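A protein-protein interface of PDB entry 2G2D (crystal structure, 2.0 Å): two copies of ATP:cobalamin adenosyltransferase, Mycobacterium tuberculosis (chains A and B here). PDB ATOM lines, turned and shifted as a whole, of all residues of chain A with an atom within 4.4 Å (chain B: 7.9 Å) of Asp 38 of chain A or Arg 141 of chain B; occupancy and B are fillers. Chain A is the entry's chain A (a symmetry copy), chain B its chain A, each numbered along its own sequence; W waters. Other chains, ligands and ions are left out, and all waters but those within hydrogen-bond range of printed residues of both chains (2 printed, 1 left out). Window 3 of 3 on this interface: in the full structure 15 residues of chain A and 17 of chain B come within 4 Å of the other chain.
The guanidinium group (NH1) of Arg 133 of chain B lies within salt-bridge range of the side-chain carboxylate (OD2) of Asp 40 of chain A. OD1 of Asp 38 of chain A lies within salt-bridge range of NH2 of Arg 141 of chain B, 3.6 Å away. The guanidinium group (NH2) of Arg 138 of chain B lies within salt-bridge range of the side-chain carboxylate (OE2) of Glu 41 of chain A, 2.8 Å away.
The side-chain carboxylate (OD1) of Asp 38 of chain B is in salt-bridge range of the guanidinium group (NH1) of Arg 138 of chain B (3.8 Å). The side-chain carboxylate (OE2) of Glu 41 of chain A is in salt-bridge range of the guanidinium group (NH2) of Arg 138 of chain A (3.0 Å). The side-chain carboxylate of Asp 38 of chain A is in salt-bridge range of the guanidinium group of Arg 138 of chain A (3.8 Å). The guanidinium group (NH1) of Arg 141 of chain B lies within hydrogen-bond range of the backbone carbonyl oxygen (O) of Arg 137 of chain B, at 3.4 Å. The side-chain hydroxyl of Ser 142 of chain A lies within hydrogen-bond range of the side-chain carboxylate of Asp 38 of chain A (2.8 Å).
CE2 of Tyr 36 of chain A touches NH1 of Arg 137 of chain B, at 3.8 Å. Arg 141 of chain B touches Ala 37 of chain A (NH1 to CB, 3.1 Å). CG2 of Thr 134 of chain B touches OD2 of Asp 40 of chain A (3.7 Å). CG of Glu 41 of chain A touches OG1 of Thr 134 of chain B, at 3.4 Å. NH1 of Arg 138 of chain A touches NE of Arg 138 of chain B (3.5 Å).
Of the printed residues of chain B, Tyr 36 of chain A touches Arg 137. Asp 38 of chain A touches one residue of chain B. Printed residues of chain B within 4 Å of Glu 41 of chain A: Thr 134 and Arg 138. Of chain A, only Ala 37 and Asp 38 come within 4 Å of Arg 141 of chain B. The nearest residue of chain A that does not touch Arg 141 of chain B is Val 34 of chain A (4.2 Å).
Of the 12 printed residues of chain A, 6 touch a printed residue of chain B. Of the 22 printed residues of chain B, 5 touch a printed residue of chain A. Among the printed residues, Asp or Glu carboxylates within 4 Å of a Lys or Arg side-chain nitrogen of the other chain: Asp 38 of chain A with Arg 141 of chain B (3.6 Å), Asp 40 of chain A with Arg 133 of chain B (2.8 Å) and Glu 41 of chain A with Arg 138 of chain B (2.8 Å).
Arg 138 of chain B touches its own counterpart, Arg 138 of chain A. Of the 8 pairs that touch across the chains among the printed residues, 1 has its exchanged pair printed and touching as well.
Water W2 lies within hydrogen-bond range of the backbone carbonyl oxygen of Thr 134 of chain B (2.8 Å) and the backbone carbonyl oxygen of Ala 37 of chain A (3.3 Å). Water W1 bridges OD2 of Asp 40 of chain A (3.0 Å) and NH1 of Arg 137 of chain B (3.4 Å).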
ATOM      1  N   VAL A  34       4.077  14.375  -0.842  1.00  0.00           N
ATOM      2  CA  VAL A  34       4.437  13.973   0.513  1.00  0.00           C
ATOM      3  C   VAL A  34       4.179  12.478   0.721  1.00  0.00           C
ATOM      4  O   VAL A  34       5.029  11.757   1.234  1.00  0.00           O
ATOM      5  CB  VAL A  34       3.643  14.771   1.563  1.00  0.00           C
ATOM      6  CG1 VAL A  34       3.946  14.237   2.965  1.00  0.00           C
ATOM      7  CG2 VAL A  34       4.013  16.245   1.479  1.00  0.00           C
ATOM      8  N   ALA A  35       2.999  12.015   0.330  1.00  0.00           N
ATOM      9  CA  ALA A  35       2.657  10.603   0.476  1.00  0.00           C
ATOM     10  C   ALA A  35       3.648   9.726  -0.301  1.00  0.00           C
ATOM     11  O   ALA A  35       4.089   8.684   0.181  1.00  0.00           O
ATOM     12  CB  ALA A  35       1.218  10.369  -0.009  1.00  0.00           C
ATOM     13  N   TYR A  36       4.005  10.153  -1.506  1.00  0.00           N
ATOM     14  CA  TYR A  36       4.947   9.395  -2.318  1.00  0.00           C
ATOM     15  C   TYR A  36       6.293   9.265  -1.599  1.00  0.00           C
ATOM     16  O   TYR A  36       6.858   8.184  -1.520  1.00  0.00           O
ATOM     17  CB  TYR A  36       5.177  10.094  -3.657  1.00  0.00           C
ATOM     18  CG  TYR A  36       6.385   9.565  -4.398  1.00  0.00           C
ATOM     19  CD1 TYR A  36       6.326   8.356  -5.089  1.00  0.00           C
ATOM     20  CD2 TYR A  36       7.597  10.250  -4.371  1.00  0.00           C
ATOM     21  CE1 TYR A  36       7.445   7.835  -5.738  1.00  0.00           C
ATOM     22  CE2 TYR A  36       8.727   9.742  -5.014  1.00  0.00           C
ATOM     23  CZ  TYR A  36       8.641   8.531  -5.696  1.00  0.00           C
ATOM     24  OH  TYR A  36       9.745   8.014  -6.340  1.00  0.00           O
ATOM     25  N   ALA A  37       6.796  10.380  -1.085  1.00  0.00           N
ATOM     26  CA  ALA A  37       8.084  10.396  -0.401  1.00  0.00           C
ATOM     27  C   ALA A  37       8.097   9.539   0.853  1.00  0.00           C
ATOM     28  O   ALA A  37       9.110   8.916   1.157  1.00  0.00           O
ATOM     29  CB  ALA A  37       8.481  11.845  -0.056  1.00  0.00           C
ATOM     30  N   ASP A  38       6.989   9.527   1.597  1.00  0.00           N
ATOM     31  CA  ASP A  38       6.921   8.720   2.808  1.00  0.00           C
ATOM     32  C   ASP A  38       6.945   7.229   2.452  1.00  0.00           C
ATOM     33  O   ASP A  38       7.493   6.422   3.206  1.00  0.00           O
ATOM     34  CB  ASP A  38       5.661   9.054   3.639  1.00  0.00           C
ATOM     35  CG  ASP A  38       5.766  10.400   4.362  1.00  0.00           C
ATOM     36  OD1 ASP A  38       6.892  10.905   4.564  1.00  0.00           O
ATOM     37  OD2 ASP A  38       4.715  10.950   4.750  1.00  0.00           O
ATOM     38  N   CYS A  39       6.354   6.858   1.313  1.00  0.00           N
ATOM     39  CA  CYS A  39       6.355   5.454   0.883  1.00  0.00           C
ATOM     40  C   CYS A  39       7.779   5.032   0.583  1.00  0.00           C
ATOM     41  O   CYS A  39       8.184   3.905   0.881  1.00  0.00           O
ATOM     42  CB  CYS A  39       5.531   5.248  -0.395  1.00  0.00           C
ATOM     43  SG  CYS A  39       3.818   4.792  -0.099  1.00  0.00           S
ATOM     44  N   ASP A  40       8.522   5.954  -0.028  1.00  0.00           N
ATOM     45  CA  ASP A  40       9.921   5.723  -0.385  1.00  0.00           C
ATOM     46  C   ASP A  40      10.736   5.559   0.927  1.00  0.00           C
ATOM     47  O   ASP A  40      11.597   4.672   1.026  1.00  0.00           O
ATOM     48  CB  ASP A  40      10.406   6.904  -1.238  1.00  0.00           C
ATOM     49  CG  ASP A  40      11.854   6.762  -1.695  1.00  0.00           C
ATOM     50  OD1 ASP A  40      12.392   5.634  -1.709  1.00  0.00           O
ATOM     51  OD2 ASP A  40      12.450   7.796  -2.053  1.00  0.00           O
ATOM     52  N   GLU A  41      10.447   6.386   1.935  1.00  0.00           N
ATOM     53  CA  GLU A  41      11.153   6.280   3.227  1.00  0.00           C
ATOM     54  C   GLU A  41      10.834   4.923   3.868  1.00  0.00           C
ATOM     55  O   GLU A  41      11.717   4.260   4.409  1.00  0.00           O
ATOM     56  CB  GLU A  41      10.747   7.421   4.182  1.00  0.00           C
ATOM     57  CG  GLU A  41      11.671   7.561   5.412  1.00  0.00           C
ATOM     58  CD  GLU A  41      11.380   8.797   6.273  1.00  0.00           C
ATOM     59  OE1 GLU A  41      10.627   9.692   5.831  1.00  0.00           O
ATOM     60  OE2 GLU A  41      11.925   8.882   7.397  1.00  0.00           O
ATOM     61  N   ALA A  42       9.571   4.505   3.816  1.00  0.00           N
ATOM     62  CA  ALA A  42       9.199   3.197   4.364  1.00  0.00           C
ATOM     63  C   ALA A  42       9.907   2.097   3.571  1.00  0.00           C
ATOM     64  O   ALA A  42      10.399   1.118   4.141  1.00  0.00           O
ATOM     65  CB  ALA A  42       7.695   2.989   4.286  1.00  0.00           C
ATOM     66  N   ARG A 138       3.576   5.954   9.382  1.00  0.00           N
ATOM     67  CA  ARG A 138       3.668   7.393   9.081  1.00  0.00           C
ATOM     68  C   ARG A 138       3.252   7.585   7.613  1.00  0.00           C
ATOM     69  O   ARG A 138       2.535   8.527   7.272  1.00  0.00           O
ATOM     70  CB  ARG A 138       5.100   7.905   9.315  1.00  0.00           C
ATOM     71  CG  ARG A 138       5.308   9.376   8.957  1.00  0.00           C
ATOM     72  CD  ARG A 138       6.311  10.064   9.895  1.00  0.00           C
ATOM     73  NE  ARG A 138       7.584   9.343  10.012  1.00  0.00           N
ATOM     74  CZ  ARG A 138       8.520   9.308   9.068  1.00  0.00           C
ATOM     75  NH1 ARG A 138       8.339   9.959   7.922  1.00  0.00           N
ATOM     76  NH2 ARG A 138       9.632   8.607   9.253  1.00  0.00           N
ATOM     77  N   ALA A 139       3.686   6.676   6.745  1.00  0.00           N
ATOM     78  CA  ALA A 139       3.321   6.745   5.326  1.00  0.00           C
ATOM     79  C   ALA A 139       1.803   6.556   5.150  1.00  0.00           C
ATOM     80  O   ALA A 139       1.189   7.182   4.274  1.00  0.00           O
ATOM     81  CB  ALA A 139       4.077   5.672   4.537  1.00  0.00           C
ATOM     82  N   SER A 142      -0.046   9.903   5.596  1.00  0.00           N
ATOM     83  CA  SER A 142       0.016  10.846   4.469  1.00  0.00           C
ATOM     84  C   SER A 142      -0.782  10.336   3.259  1.00  0.00           C
ATOM     85  O   SER A 142      -1.315  11.124   2.478  1.00  0.00           O
ATOM     86  CB  SER A 142       1.475  11.137   4.071  1.00  0.00           C
ATOM     87  OG  SER A 142       2.225   9.947   3.885  1.00  0.00           O
ATOM     88  N   VAL B  34      11.459  23.524  12.605  1.00  0.00           N
ATOM     89  CA  VAL B  34      11.184  22.228  11.996  1.00  0.00           C
ATOM     90  C   VAL B  34      12.249  21.883  10.951  1.00  0.00           C
ATOM     91  O   VAL B  34      12.785  20.780  10.938  1.00  0.00           O
ATOM     92  CB  VAL B  34       9.797  22.207  11.328  1.00  0.00           C
ATOM     93  CG1 VAL B  34       9.593  20.882  10.589  1.00  0.00           C
ATOM     94  CG2 VAL B  34       8.714  22.384  12.382  1.00  0.00           C
ATOM     95  N   ALA B  35      12.546  22.827  10.068  1.00  0.00           N
ATOM     96  CA  ALA B  35      13.554  22.603   9.035  1.00  0.00           C
ATOM     97  C   ALA B  35      14.913  22.282   9.671  1.00  0.00           C
ATOM     98  O   ALA B  35      15.633  21.392   9.219  1.00  0.00           O
ATOM     99  CB  ALA B  35      13.649  23.841   8.131  1.00  0.00           C
ATOM    100  N   ASP B  38      14.911  18.677  11.017  1.00  0.00           N
ATOM    101  CA  ASP B  38      14.941  17.666   9.970  1.00  0.00           C
ATOM    102  C   ASP B  38      16.359  17.536   9.400  1.00  0.00           C
ATOM    103  O   ASP B  38      16.770  16.441   9.012  1.00  0.00           O
ATOM    104  CB  ASP B  38      13.937  17.994   8.841  1.00  0.00           C
ATOM    105  CG  ASP B  38      12.482  17.743   9.248  1.00  0.00           C
ATOM    106  OD1 ASP B  38      12.233  16.979  10.207  1.00  0.00           O
ATOM    107  OD2 ASP B  38      11.577  18.300   8.593  1.00  0.00           O
ATOM    108  N   ARG B 133      19.133   9.116   2.226  1.00  0.00           N
ATOM    109  CA  ARG B 133      18.579   9.811   1.067  1.00  0.00           C
ATOM    110  C   ARG B 133      17.132  10.224   1.309  1.00  0.00           C
ATOM    111  O   ARG B 133      16.758  11.373   1.070  1.00  0.00           O
ATOM    112  CB  ARG B 133      18.637   8.931  -0.194  1.00  0.00           C
ATOM    113  CG  ARG B 133      17.931   9.569  -1.417  1.00  0.00           C
ATOM    114  CD  ARG B 133      18.000   8.670  -2.680  1.00  0.00           C
ATOM    115  NE  ARG B 133      17.403   7.355  -2.450  1.00  0.00           N
ATOM    116  CZ  ARG B 133      16.093   7.123  -2.371  1.00  0.00           C
ATOM    117  NH1 ARG B 133      15.214   8.115  -2.524  1.00  0.00           N
ATOM    118  NH2 ARG B 133      15.659   5.903  -2.097  1.00  0.00           N
ATOM    119  N   THR B 134      16.310   9.293   1.792  1.00  0.00           N
ATOM    120  CA  THR B 134      14.908   9.620   1.994  1.00  0.00           C
ATOM    121  C   THR B 134      14.726  10.628   3.111  1.00  0.00           C
ATOM    122  O   THR B 134      13.826  11.439   3.050  1.00  0.00           O
ATOM    123  CB  THR B 134      14.073   8.352   2.280  1.00  0.00           C
ATOM    124  OG1 THR B 134      14.508   7.743   3.500  1.00  0.00           O
ATOM    125  CG2 THR B 134      14.238   7.362   1.105  1.00  0.00           C
ATOM    126  N   VAL B 135      15.570  10.585   4.139  1.00  0.00           N
ATOM    127  CA  VAL B 135      15.430  11.565   5.210  1.00  0.00           C
ATOM    128  C   VAL B 135      15.835  12.943   4.673  1.00  0.00           C
ATOM    129  O   VAL B 135      15.199  13.946   4.975  1.00  0.00           O
ATOM    130  CB  VAL B 135      16.291  11.190   6.442  1.00  0.00           C
ATOM    131  CG1 VAL B 135      16.174  12.285   7.509  1.00  0.00           C
ATOM    132  CG2 VAL B 135      15.812   9.840   7.017  1.00  0.00           C
ATOM    133  N   VAL B 136      16.886  12.990   3.862  1.00  0.00           N
ATOM    134  CA  VAL B 136      17.314  14.262   3.279  1.00  0.00           C
ATOM    135  C   VAL B 136      16.175  14.902   2.463  1.00  0.00           C
ATOM    136  O   VAL B 136      15.960  16.115   2.513  1.00  0.00           O
ATOM    137  CB  VAL B 136      18.546  14.061   2.371  1.00  0.00           C
ATOM    138  CG1 VAL B 136      18.769  15.305   1.504  1.00  0.00           C
ATOM    139  CG2 VAL B 136      19.791  13.810   3.246  1.00  0.00           C
ATOM    140  N   ARG B 137      15.427  14.084   1.730  1.00  0.00           N
ATOM    141  CA  ARG B 137      14.326  14.607   0.915  1.00  0.00           C
ATOM    142  C   ARG B 137      13.231  15.155   1.816  1.00  0.00           C
ATOM    143  O   ARG B 137      12.538  16.104   1.450  1.00  0.00           O
ATOM    144  CB  ARG B 137      13.734  13.512   0.021  1.00  0.00           C
ATOM    145  CG  ARG B 137      14.674  12.984  -1.044  1.00  0.00           C
ATOM    146  CD  ARG B 137      13.851  12.409  -2.185  1.00  0.00           C
ATOM    147  NE  ARG B 137      13.074  13.467  -2.819  1.00  0.00           N
ATOM    148  CZ  ARG B 137      11.957  13.280  -3.513  1.00  0.00           C
ATOM    149  NH1 ARG B 137      11.464  12.060  -3.677  1.00  0.00           N
ATOM    150  NH2 ARG B 137      11.329  14.324  -4.037  1.00  0.00           N
ATOM    151  N   ARG B 138      13.055  14.545   2.987  1.00  0.00           N
ATOM    152  CA  ARG B 138      12.043  15.051   3.932  1.00  0.00           C
ATOM    153  C   ARG B 138      12.536  16.413   4.448  1.00  0.00           C
ATOM    154  O   ARG B 138      11.761  17.361   4.584  1.00  0.00           O
ATOM    155  CB  ARG B 138      11.846  14.064   5.095  1.00  0.00           C
ATOM    156  CG  ARG B 138      10.865  14.541   6.165  1.00  0.00           C
ATOM    157  CD  ARG B 138      10.060  13.382   6.771  1.00  0.00           C
ATOM    158  NE  ARG B 138      10.901  12.280   7.251  1.00  0.00           N
ATOM    159  CZ  ARG B 138      11.638  12.320   8.357  1.00  0.00           C
ATOM    160  NH1 ARG B 138      11.644  13.411   9.118  1.00  0.00           N
ATOM    161  NH2 ARG B 138      12.389  11.280   8.699  1.00  0.00           N
ATOM    162  N   ALA B 139      13.834  16.516   4.717  1.00  0.00           N
ATOM    163  CA  ALA B 139      14.415  17.780   5.183  1.00  0.00           C
ATOM    164  C   ALA B 139      14.296  18.862   4.095  1.00  0.00           C
ATOM    165  O   ALA B 139      14.080  20.043   4.404  1.00  0.00           O
ATOM    166  CB  ALA B 139      15.886  17.574   5.558  1.00  0.00           C
ATOM    167  N   GLU B 140      14.435  18.466   2.828  1.00  0.00           N
ATOM    168  CA  GLU B 140      14.331  19.430   1.726  1.00  0.00           C
ATOM    169  C   GLU B 140      12.948  20.060   1.742  1.00  0.00           C
ATOM    170  O   GLU B 140      12.818  21.265   1.563  1.00  0.00           O
ATOM    171  CB  GLU B 140      14.542  18.775   0.357  1.00  0.00           C
ATOM    172  CG  GLU B 140      14.486  19.803  -0.791  1.00  0.00           C
ATOM    173  CD  GLU B 140      14.293  19.184  -2.170  1.00  0.00           C
ATOM    174  OE1 GLU B 140      14.510  17.962  -2.324  1.00  0.00           O
ATOM    175  OE2 GLU B 140      13.932  19.935  -3.106  1.00  0.00           O
ATOM    176  N   ARG B 141      11.916  19.243   1.957  1.00  0.00           N
ATOM    177  CA  ARG B 141      10.549  19.759   1.988  1.00  0.00           C
ATOM    178  C   ARG B 141      10.332  20.811   3.064  1.00  0.00           C
ATOM    179  O   ARG B 141       9.683  21.830   2.801  1.00  0.00           O
ATOM    180  CB  ARG B 141       9.527  18.620   2.165  1.00  0.00           C
ATOM    181  CG  ARG B 141       9.542  17.602   1.029  1.00  0.00           C
ATOM    182  CD  ARG B 141       8.273  16.744   1.014  1.00  0.00           C
ATOM    183  NE  ARG B 141       8.148  15.812   2.140  1.00  0.00           N
ATOM    184  CZ  ARG B 141       8.820  14.670   2.251  1.00  0.00           C
ATOM    185  NH1 ARG B 141       9.684  14.311   1.310  1.00  0.00           N
ATOM    186  NH2 ARG B 141       8.594  13.861   3.279  1.00  0.00           N
ATOM    187  N   SER B 142      10.862  20.595   4.269  1.00  0.00           N
ATOM    188  CA  SER B 142      10.676  21.583   5.341  1.00  0.00           C
ATOM    189  C   SER B 142      11.523  22.843   5.104  1.00  0.00           C
ATOM    190  O   SER B 142      11.145  23.942   5.506  1.00  0.00           O
ATOM    191  CB  SER B 142      10.990  20.971   6.718  1.00  0.00           C
ATOM    192  OG  SER B 142      12.248  20.314   6.735  1.00  0.00           O
ATOM    193  N   ALA B 143      12.667  22.682   4.449  1.00  0.00           N
ATOM    194  CA  ALA B 143      13.517  23.829   4.133  1.00  0.00           C
ATOM    195  C   ALA B 143      12.735  24.732   3.155  1.00  0.00           C
ATOM    196  O   ALA B 143      12.726  25.950   3.300  1.00  0.00           O
ATOM    197  CB  ALA B 143      14.848  23.348   3.505  1.00  0.00           C
ATOM    198  N   TRP B 144      12.068  24.131   2.170  1.00  0.00           N
ATOM    199  CA  TRP B 144      11.267  24.898   1.208  1.00  0.00           C
ATOM    200  C   TRP B 144      10.067  25.525   1.939  1.00  0.00           C
ATOM    201  O   TRP B 144       9.654  26.642   1.633  1.00  0.00           O
ATOM    202  CB  TRP B 144      10.758  23.998   0.064  1.00  0.00           C
ATOM    203  CG  TRP B 144      11.774  23.688  -0.991  1.00  0.00           C
ATOM    204  CD1 TRP B 144      12.144  22.445  -1.444  1.00  0.00           C
ATOM    205  CD2 TRP B 144      12.557  24.635  -1.735  1.00  0.00           C
ATOM    206  NE1 TRP B 144      13.112  22.569  -2.417  1.00  0.00           N
ATOM    207  CE2 TRP B 144      13.380  23.900  -2.615  1.00  0.00           C
ATOM    208  CE3 TRP B 144      12.642  26.039  -1.739  1.00  0.00           C
ATOM    209  CZ2 TRP B 144      14.281  24.519  -3.495  1.00  0.00           C
ATOM    210  CZ3 TRP B 144      13.538  26.653  -2.617  1.00  0.00           C
ATOM    211  CH2 TRP B 144      14.345  25.890  -3.480  1.00  0.00           C
ATOM    212  N   ALA B 145       9.512  24.800   2.903  1.00  0.00           N
ATOM    213  CA  ALA B 145       8.388  25.313   3.682  1.00  0.00           C
ATOM    214  C   ALA B 145       8.836  26.517   4.516  1.00  0.00           C
ATOM    215  O   ALA B 145       8.064  27.449   4.730  1.00  0.00           O
ATOM    216  CB  ALA B 145       7.830  24.225   4.580  1.00  0.00           C
ATOM    217  N   ALA B 146      10.078  26.499   5.000  1.00  0.00           N
ATOM    218  CA  ALA B 146      10.595  27.628   5.779  1.00  0.00           C
ATOM    219  C   ALA B 146      10.656  28.859   4.868  1.00  0.00           C
ATOM    220  O   ALA B 146      10.289  29.965   5.268  1.00  0.00           O
ATOM    221  CB  ALA B 146      11.993  27.313   6.326  1.00  0.00           C
ATOM    222  N   VAL B 147      11.130  28.660   3.644  1.00  0.00           N
ATOM    223  CA  VAL B 147      11.213  29.744   2.670  1.00  0.00           C
ATOM    224  C   VAL B 147       9.815  30.312   2.407  1.00  0.00           C
ATOM    225  O   VAL B 147       9.620  31.527   2.399  1.00  0.00           O
ATOM    226  CB  VAL B 147      11.825  29.240   1.341  1.00  0.00           C
ATOM    227  CG1 VAL B 147      11.630  30.278   0.242  1.00  0.00           C
ATOM    228  CG2 VAL B 147      13.307  28.947   1.539  1.00  0.00           C
ATOM    229  N   ASP B 148       8.842  29.429   2.201  1.00  0.00           N
ATOM    230  CA  ASP B 148       7.464  29.852   1.949  1.00  0.00           C
ATOM    231  C   ASP B 148       6.887  30.683   3.086  1.00  0.00           C
ATOM    232  O   ASP B 148       6.136  31.624   2.855  1.00  0.00           O
ATOM    233  CB  ASP B 148       6.558  28.640   1.730  1.00  0.00           C
ATOM    234  CG  ASP B 148       6.630  28.104   0.316  1.00  0.00           C
ATOM    235  OD1 ASP B 148       6.430  28.895  -0.631  1.00  0.00           O
ATOM    236  OD2 ASP B 148       6.874  26.891   0.152  1.00  0.00           O
ATOM    237  N   ALA B 159      17.778  24.698   1.122  1.00  0.00           N
ATOM    238  CA  ALA B 159      16.863  23.818   0.387  1.00  0.00           C
ATOM    239  C   ALA B 159      17.508  23.267  -0.899  1.00  0.00           C
ATOM    240  O   ALA B 159      17.375  22.085  -1.215  1.00  0.00           O
ATOM    241  CB  ALA B 159      15.575  24.586   0.048  1.00  0.00           C
ATOM    242  N   LEU B 162      20.069  20.557  -0.010  1.00  0.00           N
ATOM    243  CA  LEU B 162      19.433  19.272   0.293  1.00  0.00           C
ATOM    244  C   LEU B 162      18.877  18.628  -0.974  1.00  0.00           C
ATOM    245  O   LEU B 162      18.884  17.413  -1.101  1.00  0.00           O
ATOM    246  CB  LEU B 162      18.330  19.457   1.339  1.00  0.00           C
ATOM    247  CG  LEU B 162      18.817  19.916   2.724  1.00  0.00           C
ATOM    248  CD1 LEU B 162      17.669  20.506   3.527  1.00  0.00           C
ATOM    249  CD2 LEU B 162      19.439  18.727   3.474  1.00  0.00           C
ATOM    250  N   ASN B 163      18.404  19.447  -1.912  1.00  0.00           N
ATOM    251  CA  ASN B 163      17.878  18.923  -3.172  1.00  0.00           C
ATOM    252  C   ASN B 163      18.994  18.193  -3.916  1.00  0.00           C
ATOM    253  O   ASN B 163      18.808  17.086  -4.407  1.00  0.00           O
ATOM    254  CB  ASN B 163      17.314  20.056  -4.039  1.00  0.00           C
ATOM    255  CG  ASN B 163      16.792  19.561  -5.385  1.00  0.00           C
ATOM    256  OD1 ASN B 163      17.557  19.387  -6.331  1.00  0.00           O
ATOM    257  ND2 ASN B 163      15.486  19.318  -5.466  1.00  0.00           N
HETATM  258  O   HOH W   1      11.780  10.413  -0.704  1.00  0.00           O
HETATM  259  O   HOH W   2      11.344  11.204   1.769  1.00  0.00           O
